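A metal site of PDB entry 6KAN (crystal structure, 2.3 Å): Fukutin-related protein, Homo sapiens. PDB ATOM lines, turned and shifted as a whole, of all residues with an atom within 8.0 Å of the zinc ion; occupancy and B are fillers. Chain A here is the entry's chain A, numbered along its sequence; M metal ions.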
ATOM      1  N   ARG A 235     -21.359  16.040  16.924  1.00  0.00           N
ATOM      2  CA  ARG A 235     -20.820  14.889  16.230  1.00  0.00           C
ATOM      3  C   ARG A 235     -19.305  14.917  16.134  1.00  0.00           C
ATOM      4  O   ARG A 235     -18.690  13.877  15.896  1.00  0.00           O
ATOM      5  CB  ARG A 235     -21.407  14.788  14.818  1.00  0.00           C
ATOM      6  CG  ARG A 235     -22.896  14.563  14.790  1.00  0.00           C
ATOM      7  CD  ARG A 235     -23.228  13.081  14.887  1.00  0.00           C
ATOM      8  NE  ARG A 235     -24.589  12.833  14.395  1.00  0.00           N
ATOM      9  CZ  ARG A 235     -25.685  12.986  15.123  1.00  0.00           C
ATOM     10  NH1 ARG A 235     -25.614  13.398  16.377  1.00  0.00           N
ATOM     11  NH2 ARG A 235     -26.866  12.729  14.580  1.00  0.00           N
ATOM     12  N   TRP A 246     -14.729  11.848  17.192  1.00  0.00           N
ATOM     13  CA  TRP A 246     -15.963  11.660  16.436  1.00  0.00           C
ATOM     14  C   TRP A 246     -17.023  10.939  17.257  1.00  0.00           C
ATOM     15  O   TRP A 246     -16.707  10.098  18.093  1.00  0.00           O
ATOM     16  CB  TRP A 246     -15.733  10.843  15.159  1.00  0.00           C
ATOM     17  CG  TRP A 246     -14.867  11.497  14.155  1.00  0.00           C
ATOM     18  CD1 TRP A 246     -13.543  11.260  13.946  1.00  0.00           C
ATOM     19  CD2 TRP A 246     -15.270  12.469  13.183  1.00  0.00           C
ATOM     20  NE1 TRP A 246     -13.086  12.041  12.904  1.00  0.00           N
ATOM     21  CE2 TRP A 246     -14.127  12.789  12.422  1.00  0.00           C
ATOM     22  CE3 TRP A 246     -16.475  13.105  12.896  1.00  0.00           C
ATOM     23  CZ2 TRP A 246     -14.148  13.737  11.375  1.00  0.00           C
ATOM     24  CZ3 TRP A 246     -16.502  14.065  11.861  1.00  0.00           C
ATOM     25  CH2 TRP A 246     -15.344  14.361  11.114  1.00  0.00           C
ATOM     26  N   PHE A 247     -18.290  11.275  16.979  1.00  0.00           N
ATOM     27  CA  PHE A 247     -19.437  10.754  17.723  1.00  0.00           C
ATOM     28  C   PHE A 247     -20.627  10.525  16.793  1.00  0.00           C
ATOM     29  O   PHE A 247     -21.773  10.630  17.231  1.00  0.00           O
ATOM     30  CB  PHE A 247     -19.809  11.681  18.890  1.00  0.00           C
ATOM     31  CG  PHE A 247     -18.675  11.884  19.875  1.00  0.00           C
ATOM     32  CD1 PHE A 247     -18.486  10.993  20.929  1.00  0.00           C
ATOM     33  CD2 PHE A 247     -17.767  12.918  19.704  1.00  0.00           C
ATOM     34  CE1 PHE A 247     -17.425  11.170  21.821  1.00  0.00           C
ATOM     35  CE2 PHE A 247     -16.706  13.095  20.596  1.00  0.00           C
ATOM     36  CZ  PHE A 247     -16.536  12.211  21.660  1.00  0.00           C
ATOM     37  N   GLY A 248     -20.370  10.229  15.528  1.00  0.00           N
ATOM     38  CA  GLY A 248     -21.417  10.077  14.545  1.00  0.00           C
ATOM     39  C   GLY A 248     -21.462   8.690  13.928  1.00  0.00           C
ATOM     40  O   GLY A 248     -21.378   7.685  14.632  1.00  0.00           O
ATOM     41  N   CYS A 249     -21.623   8.634  12.615  1.00  0.00           N
ATOM     42  CA  CYS A 249     -21.681   7.371  11.905  1.00  0.00           C
ATOM     43  C   CYS A 249     -20.276   6.989  11.410  1.00  0.00           C
ATOM     44  O   CYS A 249     -19.336   7.789  11.468  1.00  0.00           O
ATOM     45  CB  CYS A 249     -22.684   7.472  10.760  1.00  0.00           C
ATOM     46  SG  CYS A 249     -22.107   8.552   9.463  1.00  0.00           S
ATOM     47  N   ASN A 250     -20.122   5.749  10.946  1.00  0.00           N
ATOM     48  CA  ASN A 250     -18.829   5.260  10.427  1.00  0.00           C
ATOM     49  C   ASN A 250     -19.087   4.055   9.528  1.00  0.00           C
ATOM     50  O   ASN A 250     -20.232   3.702   9.237  1.00  0.00           O
ATOM     51  CB  ASN A 250     -17.851   4.888  11.566  1.00  0.00           C
ATOM     52  CG  ASN A 250     -18.421   3.828  12.510  1.00  0.00           C
ATOM     53  OD1 ASN A 250     -18.738   2.699  12.105  1.00  0.00           O
ATOM     54  ND2 ASN A 250     -18.575   4.193  13.784  1.00  0.00           N
ATOM     55  N   THR A 253     -21.606   1.430  10.959  1.00  0.00           N
ATOM     56  CA  THR A 253     -22.920   1.816  11.438  1.00  0.00           C
ATOM     57  C   THR A 253     -23.810   2.264  10.274  1.00  0.00           C
ATOM     58  O   THR A 253     -23.394   2.351   9.115  1.00  0.00           O
ATOM     59  CB  THR A 253     -22.832   2.937  12.482  1.00  0.00           C
ATOM     60  OG1 THR A 253     -22.628   4.187  11.815  1.00  0.00           O
ATOM     61  CG2 THR A 253     -21.702   2.660  13.457  1.00  0.00           C
ATOM     62  N   THR A 254     -25.059   2.544  10.595  1.00  0.00           N
ATOM     63  CA  THR A 254     -25.941   3.217   9.664  1.00  0.00           C
ATOM     64  C   THR A 254     -25.537   4.695   9.543  1.00  0.00           C
ATOM     65  O   THR A 254     -24.904   5.260  10.427  1.00  0.00           O
ATOM     66  CB  THR A 254     -27.388   3.076  10.159  1.00  0.00           C
ATOM     67  OG1 THR A 254     -28.281   3.580   9.173  1.00  0.00           O
ATOM     68  CG2 THR A 254     -27.577   3.830  11.477  1.00  0.00           C
ATOM     69  N   ARG A 255     -25.865   5.313   8.408  1.00  0.00           N
ATOM     70  CA  ARG A 255     -25.625   6.756   8.320  1.00  0.00           C
ATOM     71  C   ARG A 255     -26.576   7.500   9.262  1.00  0.00           C
ATOM     72  O   ARG A 255     -27.613   6.974   9.680  1.00  0.00           O
ATOM     73  CB  ARG A 255     -25.798   7.261   6.882  1.00  0.00           C
ATOM     74  CG  ARG A 255     -27.238   7.528   6.431  1.00  0.00           C
ATOM     75  CD  ARG A 255     -27.317   7.690   4.933  1.00  0.00           C
ATOM     76  NE  ARG A 255     -28.689   7.759   4.424  1.00  0.00           N
ATOM     77  CZ  ARG A 255     -28.992   7.955   3.132  1.00  0.00           C
ATOM     78  NH1 ARG A 255     -28.027   8.107   2.240  1.00  0.00           N
ATOM     79  NH2 ARG A 255     -30.260   8.000   2.733  1.00  0.00           N
ATOM     80  N   CYS A 256     -26.202   8.734   9.625  1.00  0.00           N
ATOM     81  CA  CYS A 256     -26.915   9.436  10.692  1.00  0.00           C
ATOM     82  C   CYS A 256     -28.394   9.616  10.371  1.00  0.00           C
ATOM     83  O   CYS A 256     -29.260   9.364  11.211  1.00  0.00           O
ATOM     84  CB  CYS A 256     -26.265  10.782  10.965  1.00  0.00           C
ATOM     85  SG  CYS A 256     -24.646  10.630  11.762  1.00  0.00           S
ATOM     86  N   PHE A 257     -28.699  10.037   9.156  1.00  0.00           N
ATOM     87  CA  PHE A 257     -30.069  10.451   8.890  1.00  0.00           C
ATOM     88  C   PHE A 257     -30.887   9.347   8.257  1.00  0.00           C
ATOM     89  O   PHE A 257     -32.052   9.574   7.930  1.00  0.00           O
ATOM     90  CB  PHE A 257     -30.090  11.725   8.017  1.00  0.00           C
ATOM     91  CG  PHE A 257     -29.265  11.629   6.761  1.00  0.00           C
ATOM     92  CD1 PHE A 257     -27.899  11.929   6.775  1.00  0.00           C
ATOM     93  CD2 PHE A 257     -29.843  11.259   5.559  1.00  0.00           C
ATOM     94  CE1 PHE A 257     -27.141  11.850   5.629  1.00  0.00           C
ATOM     95  CE2 PHE A 257     -29.097  11.173   4.398  1.00  0.00           C
ATOM     96  CZ  PHE A 257     -27.734  11.457   4.438  1.00  0.00           C
ATOM     97  N   THR A 274     -25.589  19.023   7.057  1.00  0.00           N
ATOM     98  CA  THR A 274     -25.199  17.612   7.015  1.00  0.00           C
ATOM     99  C   THR A 274     -24.232  17.312   8.152  1.00  0.00           C
ATOM    100  O   THR A 274     -23.282  18.071   8.373  1.00  0.00           O
ATOM    101  CB  THR A 274     -24.564  17.282   5.684  1.00  0.00           C
ATOM    102  OG1 THR A 274     -25.450  17.679   4.612  1.00  0.00           O
ATOM    103  CG2 THR A 274     -24.301  15.779   5.569  1.00  0.00           C
ATOM    104  N   PRO A 275     -24.443  16.236   8.913  1.00  0.00           N
ATOM    105  CA  PRO A 275     -23.487  15.878   9.966  1.00  0.00           C
ATOM    106  C   PRO A 275     -22.087  15.745   9.389  1.00  0.00           C
ATOM    107  O   PRO A 275     -21.910  15.331   8.231  1.00  0.00           O
ATOM    108  CB  PRO A 275     -24.016  14.540  10.491  1.00  0.00           C
ATOM    109  CG  PRO A 275     -25.514  14.681  10.299  1.00  0.00           C
ATOM    110  CD  PRO A 275     -25.656  15.395   8.961  1.00  0.00           C
ATOM    111  N   PRO A 276     -21.069  16.115  10.161  1.00  0.00           N
ATOM    112  CA  PRO A 276     -19.709  16.114   9.602  1.00  0.00           C
ATOM    113  C   PRO A 276     -19.112  14.714   9.466  1.00  0.00           C
ATOM    114  O   PRO A 276     -18.202  14.510   8.647  1.00  0.00           O
ATOM    115  CB  PRO A 276     -18.910  16.977  10.589  1.00  0.00           C
ATOM    116  CG  PRO A 276     -19.671  16.851  11.909  1.00  0.00           C
ATOM    117  CD  PRO A 276     -21.133  16.674  11.525  1.00  0.00           C
ATOM    118  N   CYS A 277     -19.596  13.748  10.242  1.00  0.00           N
ATOM    119  CA  CYS A 277     -19.241  12.358   9.986  1.00  0.00           C
ATOM    120  C   CYS A 277     -19.795  11.906   8.645  1.00  0.00           C
ATOM    121  O   CYS A 277     -19.140  11.144   7.924  1.00  0.00           O
ATOM    122  CB  CYS A 277     -19.769  11.463  11.099  1.00  0.00           C
ATOM    123  SG  CYS A 277     -21.523  11.808  11.432  1.00  0.00           S
ATOM    124  N   CYS A 278     -21.009  12.348   8.287  1.00  0.00           N
ATOM    125  CA  CYS A 278     -21.567  11.962   6.997  1.00  0.00           C
ATOM    126  C   CYS A 278     -20.813  12.627   5.842  1.00  0.00           C
ATOM    127  O   CYS A 278     -20.593  12.020   4.804  1.00  0.00           O
ATOM    128  CB  CYS A 278     -23.038  12.319   6.932  1.00  0.00           C
ATOM    129  SG  CYS A 278     -24.137  11.510   8.137  1.00  0.00           S
ATOM    130  N   LEU A 279     -20.436  13.899   6.008  1.00  0.00           N
ATOM    131  CA  LEU A 279     -19.618  14.544   4.991  1.00  0.00           C
ATOM    132  C   LEU A 279     -18.260  13.865   4.872  1.00  0.00           C
ATOM    133  O   LEU A 279     -17.751  13.650   3.768  1.00  0.00           O
ATOM    134  CB  LEU A 279     -19.467  16.041   5.310  1.00  0.00           C
ATOM    135  CG  LEU A 279     -20.712  16.901   5.102  1.00  0.00           C
ATOM    136  CD1 LEU A 279     -20.513  18.350   5.679  1.00  0.00           C
ATOM    137  CD2 LEU A 279     -21.121  16.928   3.625  1.00  0.00           C
ATOM    138  N   ARG A 280     -17.681  13.471   6.014  1.00  0.00           N
ATOM    139  CA  ARG A 280     -16.375  12.811   5.992  1.00  0.00           C
ATOM    140  C   ARG A 280     -16.428  11.507   5.203  1.00  0.00           C
ATOM    141  O   ARG A 280     -15.567  11.236   4.361  1.00  0.00           O
ATOM    142  CB  ARG A 280     -15.882  12.574   7.431  1.00  0.00           C
ATOM    143  CG  ARG A 280     -14.425  12.117   7.544  1.00  0.00           C
ATOM    144  CD  ARG A 280     -14.244  11.211   8.760  1.00  0.00           C
ATOM    145  NE  ARG A 280     -15.124  10.052   8.662  1.00  0.00           N
ATOM    146  CZ  ARG A 280     -14.869   9.004   7.888  1.00  0.00           C
ATOM    147  NH1 ARG A 280     -13.754   8.945   7.165  1.00  0.00           N
ATOM    148  NH2 ARG A 280     -15.736   7.992   7.842  1.00  0.00           N
ATOM    149  N   ALA A 281     -17.460  10.688   5.442  1.00  0.00           N
ATOM    150  CA  ALA A 281     -17.592   9.457   4.662  1.00  0.00           C
ATOM    151  C   ALA A 281     -17.813   9.763   3.185  1.00  0.00           C
ATOM    152  O   ALA A 281     -17.333   9.037   2.321  1.00  0.00           O
ATOM    153  CB  ALA A 281     -18.740   8.617   5.217  1.00  0.00           C
ATOM    154  N   ASN A 371     -23.607   1.555   5.874  1.00  0.00           N
ATOM    155  CA  ASN A 371     -23.653   3.010   5.821  1.00  0.00           C
ATOM    156  C   ASN A 371     -23.899   3.446   4.378  1.00  0.00           C
ATOM    157  O   ASN A 371     -22.975   3.418   3.554  1.00  0.00           O
ATOM    158  CB  ASN A 371     -22.360   3.617   6.359  1.00  0.00           C
ATOM    159  CG  ASN A 371     -22.448   5.130   6.499  1.00  0.00           C
ATOM    160  OD1 ASN A 371     -23.048   5.796   5.642  1.00  0.00           O
ATOM    161  ND2 ASN A 371     -21.862   5.676   7.578  1.00  0.00           N
ATOM    162  N   LEU A 373     -24.277   6.158   2.641  1.00  0.00           N
ATOM    163  CA  LEU A 373     -23.843   7.372   1.965  1.00  0.00           C
ATOM    164  C   LEU A 373     -23.159   6.958   0.666  1.00  0.00           C
ATOM    165  O   LEU A 373     -22.456   5.942   0.619  1.00  0.00           O
ATOM    166  CB  LEU A 373     -22.924   8.167   2.868  1.00  0.00           C
ATOM    167  CG  LEU A 373     -23.545   8.727   4.154  1.00  0.00           C
ATOM    168  CD1 LEU A 373     -22.455   8.938   5.182  1.00  0.00           C
ATOM    169  CD2 LEU A 373     -24.320  10.041   3.887  1.00  0.00           C
HETATM  170 ZN    ZN M   1     -22.954  10.719  10.037  1.00  0.00          ZN
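The side-chain sulfur of Cys 249 sits close to the side-chain amide nitrogen of Asn 371, 3.4 Å away.
The side-chain sulfur (SG) of Cys 256 sits close to the guanidinium group (NE) of Arg 235, 3.4 Å away.
Pro 275 touches the zinc ion.
Five residues have an atom within 4 Å of the zinc ion: Cys 249, Cys 256, Pro 275, Cys 277 and Cys 278.
The nearest printed residue that does not touch the zinc ion is Gly 248 (4.6 Å).
The zinc ion is bound by SG of Cys 277 (2.3 Å).
SG of Cys 278 binds the zinc ion (2.4 Å).
The side-chain sulfur (SG) of Cys 249 binds the zinc ion (2.4 Å).
The side-chain sulfur (SG) of Cys 256 is bound to the zinc ion.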
